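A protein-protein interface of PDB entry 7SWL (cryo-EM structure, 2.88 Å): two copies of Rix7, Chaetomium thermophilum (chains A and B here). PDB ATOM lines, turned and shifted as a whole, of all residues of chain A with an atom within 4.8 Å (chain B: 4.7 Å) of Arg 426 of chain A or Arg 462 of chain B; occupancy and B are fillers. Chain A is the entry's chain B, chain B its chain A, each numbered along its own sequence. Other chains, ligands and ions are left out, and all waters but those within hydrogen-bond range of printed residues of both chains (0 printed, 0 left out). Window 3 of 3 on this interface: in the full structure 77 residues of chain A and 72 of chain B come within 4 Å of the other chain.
The side-chain sulfur (SD) of Met 465 of chain B sits close to the backbone carbonyl oxygen (O) of Arg 426 of chain A (3.7 Å). The guanidinium group of Arg 426 of chain A lies within salt-bridge range of the side-chain carboxylate of Asp 420 of chain B, at 3.0 Å. The side-chain amide nitrogen (ND2) of Asn 461 of chain B sits close to the guanidinium group (NH2) of Arg 426 of chain A, at 3.0 Å. OD2 of Asp 420 of chain B is in hydrogen-bond range of ND2 of Asn 439 of chain A. NH1 of Arg 462 of chain B sits at hydrogen-bond distance from O of Arg 426 of chain A.
ND2 of Asn 439 of chain A lies close to NH1 of Arg 426 of chain A. OD1 of Asp 420 of chain B is in hydrogen-bond range of OG1 of Thr 460 of chain B (2.6 Å). NE of Arg 426 of chain A lies within salt-bridge range of OD2 of Asp 467 of chain A (2.7 Å). OD1 of Asn 461 of chain B lies close to OE1 of Gln 418 of chain B, 3.2 Å away. The side-chain hydroxyl (OG1) of Thr 460 of chain B is in hydrogen-bond range of the backbone NH (N) of Arg 462 of chain B, 3.3 Å away. The guanidinium group (NH2) of Arg 462 of chain B is in salt-bridge range of the side-chain carboxylate (OD2) of Asp 464 of chain B (3.0 Å).
Asn 439 of chain A touches Gln 418 of chain B. NE2 of Gln 418 of chain B touches CB of Leu 442 of chain A, 3.8 Å away. Asn 461 of chain B touches Ala 469 of chain A.
Printed residues of chain B within 4 Å of Asn 439 of chain A: Gln 418 and Asp 420. Printed residues of chain A within 4 Å of Asp 420 of chain B: Arg 426 and Asn 439. Of the printed residues of chain A, Asn 461 of chain B touches Arg 426 (3.0 Å) and Ala 469 (3.2 Å). Arg 462 of chain B touches just one residue of chain A: Arg 426 (2.8 Å). Pro 463 of chain B touches none of the printed residues of chain A. The nearest residue of chain B that does not touch Arg 426 of chain A is Gln 418 of chain B (4.2 Å). The nearest printed residue of chain B that does not touch Leu 442 of chain A is Asn 461 of chain B (4.8 Å).
Of the 10 printed residues of chain B, 5 touch a printed residue of chain A. Printed residues of chain B that touch a printed residue of chain A: Gln 418, Asp 420, Asn 461, Arg 462 and Met 465. Of the 11 printed residues of chain A, 4 touch a printed residue of chain B. Printed residues of chain A that touch a printed residue of chain B: Arg 426, Asn 439, Leu 442 and Ala 469. Among the printed residues, 8 pairs touch across the chains. Among the printed residues, Asp or Glu carboxylates within 4 Å of a Lys or Arg side-chain nitrogen of the other chain: Arg 426 of chain A with Asp 420 of chain B (3.0 Å).
No position is printed for both chains.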
ATOM      1  N   PRO A 424       2.025   1.804  -4.883  1.00  0.00           N
ATOM      2  CA  PRO A 424       1.190   1.432  -6.027  1.00  0.00           C
ATOM      3  C   PRO A 424       2.025   0.797  -7.128  1.00  0.00           C
ATOM      4  O   PRO A 424       3.251   0.909  -7.160  1.00  0.00           O
ATOM      5  CB  PRO A 424       0.597   2.768  -6.477  1.00  0.00           C
ATOM      6  CG  PRO A 424       1.623   3.763  -6.086  1.00  0.00           C
ATOM      7  CD  PRO A 424       2.242   3.259  -4.814  1.00  0.00           C
ATOM      8  N   ARG A 425       1.337   0.113  -8.039  1.00  0.00           N
ATOM      9  CA  ARG A 425       2.023  -0.543  -9.144  1.00  0.00           C
ATOM     10  C   ARG A 425       2.725   0.486 -10.018  1.00  0.00           C
ATOM     11  O   ARG A 425       2.157   1.529 -10.351  1.00  0.00           O
ATOM     12  CB  ARG A 425       1.038  -1.359  -9.976  1.00  0.00           C
ATOM     13  CG  ARG A 425       0.585  -2.637  -9.304  1.00  0.00           C
ATOM     14  CD  ARG A 425      -0.198  -3.526 -10.251  1.00  0.00           C
ATOM     15  NE  ARG A 425      -0.515  -4.811  -9.639  1.00  0.00           N
ATOM     16  CZ  ARG A 425      -1.124  -5.811 -10.262  1.00  0.00           C
ATOM     17  NH1 ARG A 425      -1.503  -5.710 -11.525  1.00  0.00           N
ATOM     18  NH2 ARG A 425      -1.359  -6.940  -9.600  1.00  0.00           N
ATOM     19  N   ARG A 426       3.966   0.188 -10.387  1.00  0.00           N
ATOM     20  CA  ARG A 426       4.778   1.097 -11.190  1.00  0.00           C
ATOM     21  C   ARG A 426       4.288   1.046 -12.631  1.00  0.00           C
ATOM     22  O   ARG A 426       4.653   0.152 -13.395  1.00  0.00           O
ATOM     23  CB  ARG A 426       6.252   0.726 -11.093  1.00  0.00           C
ATOM     24  CG  ARG A 426       6.873   0.995  -9.735  1.00  0.00           C
ATOM     25  CD  ARG A 426       8.260   0.394  -9.645  1.00  0.00           C
ATOM     26  NE  ARG A 426       8.217  -1.060  -9.731  1.00  0.00           N
ATOM     27  CZ  ARG A 426       9.285  -1.838  -9.835  1.00  0.00           C
ATOM     28  NH1 ARG A 426      10.505  -1.333  -9.878  1.00  0.00           N
ATOM     29  NH2 ARG A 426       9.124  -3.155  -9.901  1.00  0.00           N
ATOM     30  N   ASP A 427       3.451   2.007 -13.000  1.00  0.00           N
ATOM     31  CA  ASP A 427       2.964   2.167 -14.360  1.00  0.00           C
ATOM     32  C   ASP A 427       3.559   3.428 -14.972  1.00  0.00           C
ATOM     33  O   ASP A 427       4.205   4.233 -14.297  1.00  0.00           O
ATOM     34  CB  ASP A 427       1.432   2.231 -14.390  1.00  0.00           C
ATOM     35  CG  ASP A 427       0.784   0.950 -13.906  1.00  0.00           C
ATOM     36  OD1 ASP A 427       1.348  -0.136 -14.156  1.00  0.00           O
ATOM     37  OD2 ASP A 427      -0.291   1.029 -13.274  1.00  0.00           O
ATOM     38  N   ASP A 428       3.332   3.594 -16.276  1.00  0.00           N
ATOM     39  CA  ASP A 428       3.827   4.775 -16.969  1.00  0.00           C
ATOM     40  C   ASP A 428       3.082   6.043 -16.572  1.00  0.00           C
ATOM     41  O   ASP A 428       3.571   7.142 -16.852  1.00  0.00           O
ATOM     42  CB  ASP A 428       3.734   4.572 -18.483  1.00  0.00           C
ATOM     43  CG  ASP A 428       4.676   5.479 -19.252  1.00  0.00           C
ATOM     44  OD1 ASP A 428       5.523   6.136 -18.613  1.00  0.00           O
ATOM     45  OD2 ASP A 428       4.571   5.532 -20.495  1.00  0.00           O
ATOM     46  N   LEU A 430       2.210   6.655 -13.314  1.00  0.00           N
ATOM     47  CA  LEU A 430       2.369   6.791 -11.871  1.00  0.00           C
ATOM     48  C   LEU A 430       3.205   8.001 -11.476  1.00  0.00           C
ATOM     49  O   LEU A 430       3.374   8.248 -10.276  1.00  0.00           O
ATOM     50  CB  LEU A 430       3.000   5.519 -11.294  1.00  0.00           C
ATOM     51  CG  LEU A 430       2.795   5.258  -9.801  1.00  0.00           C
ATOM     52  CD1 LEU A 430       1.359   4.856  -9.532  1.00  0.00           C
ATOM     53  CD2 LEU A 430       3.761   4.205  -9.291  1.00  0.00           C
ATOM     54  N   VAL A 438       8.404   3.875  -4.286  1.00  0.00           N
ATOM     55  CA  VAL A 438       8.239   2.430  -4.406  1.00  0.00           C
ATOM     56  C   VAL A 438       9.594   1.750  -4.530  1.00  0.00           C
ATOM     57  O   VAL A 438       9.856   0.734  -3.878  1.00  0.00           O
ATOM     58  CB  VAL A 438       7.326   2.092  -5.598  1.00  0.00           C
ATOM     59  CG1 VAL A 438       7.140   0.591  -5.713  1.00  0.00           C
ATOM     60  CG2 VAL A 438       5.988   2.785  -5.453  1.00  0.00           C
ATOM     61  N   ASN A 439      10.478   2.301  -5.363  1.00  0.00           N
ATOM     62  CA  ASN A 439      11.800   1.709  -5.540  1.00  0.00           C
ATOM     63  C   ASN A 439      12.637   1.825  -4.273  1.00  0.00           C
ATOM     64  O   ASN A 439      13.413   0.918  -3.955  1.00  0.00           O
ATOM     65  CB  ASN A 439      12.512   2.363  -6.720  1.00  0.00           C
ATOM     66  CG  ASN A 439      11.962   1.907  -8.054  1.00  0.00           C
ATOM     67  OD1 ASN A 439      11.356   2.684  -8.789  1.00  0.00           O
ATOM     68  ND2 ASN A 439      12.172   0.640  -8.374  1.00  0.00           N
ATOM     69  N   LEU A 442      11.652  -0.814  -2.134  1.00  0.00           N
ATOM     70  CA  LEU A 442      12.138  -2.093  -2.638  1.00  0.00           C
ATOM     71  C   LEU A 442      13.537  -2.396  -2.121  1.00  0.00           C
ATOM     72  O   LEU A 442      13.828  -3.532  -1.733  1.00  0.00           O
ATOM     73  CB  LEU A 442      12.122  -2.097  -4.166  1.00  0.00           C
ATOM     74  CG  LEU A 442      10.766  -2.176  -4.866  1.00  0.00           C
ATOM     75  CD1 LEU A 442      10.942  -2.099  -6.365  1.00  0.00           C
ATOM     76  CD2 LEU A 442      10.055  -3.448  -4.484  1.00  0.00           C
ATOM     77  N   ASP A 467       2.464  -3.016  -5.872  1.00  0.00           N
ATOM     78  CA  ASP A 467       3.465  -3.441  -6.840  1.00  0.00           C
ATOM     79  C   ASP A 467       3.790  -4.917  -6.656  1.00  0.00           C
ATOM     80  O   ASP A 467       3.896  -5.413  -5.533  1.00  0.00           O
ATOM     81  CB  ASP A 467       4.731  -2.599  -6.695  1.00  0.00           C
ATOM     82  CG  ASP A 467       5.659  -2.736  -7.879  1.00  0.00           C
ATOM     83  OD1 ASP A 467       5.247  -3.331  -8.895  1.00  0.00           O
ATOM     84  OD2 ASP A 467       6.803  -2.247  -7.798  1.00  0.00           O
ATOM     85  N   ALA A 469       6.522  -6.409  -7.248  1.00  0.00           N
ATOM     86  CA  ALA A 469       7.843  -6.622  -6.670  1.00  0.00           C
ATOM     87  C   ALA A 469       7.803  -6.583  -5.151  1.00  0.00           C
ATOM     88  O   ALA A 469       8.566  -7.297  -4.495  1.00  0.00           O
ATOM     89  CB  ALA A 469       8.820  -5.578  -7.198  1.00  0.00           C
ATOM     90  N   GLN B 418      17.753  -1.239  -8.515  1.00  0.00           N
ATOM     91  CA  GLN B 418      16.481  -0.654  -8.938  1.00  0.00           C
ATOM     92  C   GLN B 418      16.729   0.609  -9.759  1.00  0.00           C
ATOM     93  O   GLN B 418      16.268   1.703  -9.435  1.00  0.00           O
ATOM     94  CB  GLN B 418      15.573  -0.364  -7.740  1.00  0.00           C
ATOM     95  CG  GLN B 418      15.475  -1.492  -6.728  1.00  0.00           C
ATOM     96  CD  GLN B 418      14.720  -2.696  -7.244  1.00  0.00           C
ATOM     97  OE1 GLN B 418      14.172  -2.684  -8.344  1.00  0.00           O
ATOM     98  NE2 GLN B 418      14.683  -3.750  -6.440  1.00  0.00           N
ATOM     99  N   ASP B 420      15.667   1.633 -12.540  1.00  0.00           N
ATOM    100  CA  ASP B 420      14.574   2.277 -13.257  1.00  0.00           C
ATOM    101  C   ASP B 420      14.087   3.546 -12.570  1.00  0.00           C
ATOM    102  O   ASP B 420      13.391   4.343 -13.207  1.00  0.00           O
ATOM    103  CB  ASP B 420      13.408   1.303 -13.441  1.00  0.00           C
ATOM    104  CG  ASP B 420      13.091   0.523 -12.183  1.00  0.00           C
ATOM    105  OD1 ASP B 420      14.009  -0.108 -11.623  1.00  0.00           O
ATOM    106  OD2 ASP B 420      11.920   0.541 -11.752  1.00  0.00           O
ATOM    107  N   THR B 460      17.308  -4.012 -12.524  1.00  0.00           N
ATOM    108  CA  THR B 460      15.934  -3.538 -12.533  1.00  0.00           C
ATOM    109  C   THR B 460      15.037  -4.674 -12.994  1.00  0.00           C
ATOM    110  O   THR B 460      15.424  -5.465 -13.855  1.00  0.00           O
ATOM    111  CB  THR B 460      15.759  -2.314 -13.442  1.00  0.00           C
ATOM    112  OG1 THR B 460      14.376  -1.948 -13.492  1.00  0.00           O
ATOM    113  CG2 THR B 460      16.254  -2.606 -14.850  1.00  0.00           C
ATOM    114  N   ASN B 461      13.849  -4.761 -12.404  1.00  0.00           N
ATOM    115  CA  ASN B 461      12.883  -5.784 -12.774  1.00  0.00           C
ATOM    116  C   ASN B 461      11.802  -5.263 -13.707  1.00  0.00           C
ATOM    117  O   ASN B 461      10.926  -6.033 -14.107  1.00  0.00           O
ATOM    118  CB  ASN B 461      12.245  -6.390 -11.522  1.00  0.00           C
ATOM    119  CG  ASN B 461      11.785  -5.341 -10.540  1.00  0.00           C
ATOM    120  OD1 ASN B 461      12.382  -4.272 -10.427  1.00  0.00           O
ATOM    121  ND2 ASN B 461      10.718  -5.643  -9.817  1.00  0.00           N
ATOM    122  N   ARG B 462      11.842  -3.981 -14.063  1.00  0.00           N
ATOM    123  CA  ARG B 462      10.922  -3.393 -15.033  1.00  0.00           C
ATOM    124  C   ARG B 462      11.749  -2.644 -16.067  1.00  0.00           C
ATOM    125  O   ARG B 462      11.878  -1.415 -16.006  1.00  0.00           O
ATOM    126  CB  ARG B 462       9.901  -2.479 -14.355  1.00  0.00           C
ATOM    127  CG  ARG B 462       9.109  -3.170 -13.262  1.00  0.00           C
ATOM    128  CD  ARG B 462       7.720  -2.581 -13.089  1.00  0.00           C
ATOM    129  NE  ARG B 462       6.812  -2.986 -14.155  1.00  0.00           N
ATOM    130  CZ  ARG B 462       6.339  -2.173 -15.088  1.00  0.00           C
ATOM    131  NH1 ARG B 462       6.655  -0.890 -15.109  1.00  0.00           N
ATOM    132  NH2 ARG B 462       5.524  -2.657 -16.020  1.00  0.00           N
ATOM    133  N   PRO B 463      12.335  -3.361 -17.032  1.00  0.00           N
ATOM    134  CA  PRO B 463      13.163  -2.696 -18.050  1.00  0.00           C
ATOM    135  C   PRO B 463      12.379  -1.796 -18.987  1.00  0.00           C
ATOM    136  O   PRO B 463      12.997  -1.061 -19.767  1.00  0.00           O
ATOM    137  CB  PRO B 463      13.790  -3.869 -18.816  1.00  0.00           C
ATOM    138  CG  PRO B 463      13.595  -5.063 -17.939  1.00  0.00           C
ATOM    139  CD  PRO B 463      12.332  -4.821 -17.197  1.00  0.00           C
ATOM    140  N   ASP B 464      11.049  -1.834 -18.950  1.00  0.00           N
ATOM    141  CA  ASP B 464      10.245  -0.973 -19.803  1.00  0.00           C
ATOM    142  C   ASP B 464      10.100   0.440 -19.255  1.00  0.00           C
ATOM    143  O   ASP B 464       9.558   1.302 -19.953  1.00  0.00           O
ATOM    144  CB  ASP B 464       8.860  -1.589 -20.017  1.00  0.00           C
ATOM    145  CG  ASP B 464       8.279  -2.175 -18.746  1.00  0.00           C
ATOM    146  OD1 ASP B 464       9.019  -2.859 -18.011  1.00  0.00           O
ATOM    147  OD2 ASP B 464       7.081  -1.951 -18.481  1.00  0.00           O
ATOM    148  N   MET B 465      10.560   0.699 -18.032  1.00  0.00           N
ATOM    149  CA  MET B 465      10.513   2.033 -17.450  1.00  0.00           C
ATOM    150  C   MET B 465      11.875   2.706 -17.391  1.00  0.00           C
ATOM    151  O   MET B 465      11.970   3.833 -16.895  1.00  0.00           O
ATOM    152  CB  MET B 465       9.914   1.981 -16.042  1.00  0.00           C
ATOM    153  CG  MET B 465       8.436   1.659 -16.003  1.00  0.00           C
ATOM    154  SD  MET B 465       7.778   1.843 -14.340  1.00  0.00           S
ATOM    155  CE  MET B 465       9.034   0.979 -13.400  1.00  0.00           C
ATOM    156  N   ILE B 466      12.920   2.055 -17.874  1.00  0.00           N
ATOM    157  CA  ILE B 466      14.262   2.618 -17.859  1.00  0.00           C
ATOM    158  C   ILE B 466      14.528   3.255 -19.214  1.00  0.00           C
ATOM    159  O   ILE B 466      14.035   2.795 -20.251  1.00  0.00           O
ATOM    160  CB  ILE B 466      15.318   1.547 -17.507  1.00  0.00           C
ATOM    161  CG1 ILE B 466      16.661   2.197 -17.178  1.00  0.00           C
ATOM    162  CG2 ILE B 466      15.479   0.546 -18.634  1.00  0.00           C
ATOM    163  CD1 ILE B 466      17.713   1.211 -16.736  1.00  0.00           C
ATOM    164  N   LYS B 612       5.430 -11.005 -18.607  1.00  0.00           N
ATOM    165  CA  LYS B 612       5.515  -9.549 -18.583  1.00  0.00           C
ATOM    166  C   LYS B 612       6.952  -9.079 -18.392  1.00  0.00           C
ATOM    167  O   LYS B 612       7.390  -8.118 -19.034  1.00  0.00           O
ATOM    168  CB  LYS B 612       4.620  -8.996 -17.475  1.00  0.00           C
ATOM    169  CG  LYS B 612       4.933  -7.565 -17.076  1.00  0.00           C
ATOM    170  CD  LYS B 612       4.202  -7.176 -15.803  1.00  0.00           C
ATOM    171  CE  LYS B 612       4.635  -5.803 -15.317  1.00  0.00           C
ATOM    172  NZ  LYS B 612       3.944  -5.424 -14.056  1.00  0.00           N
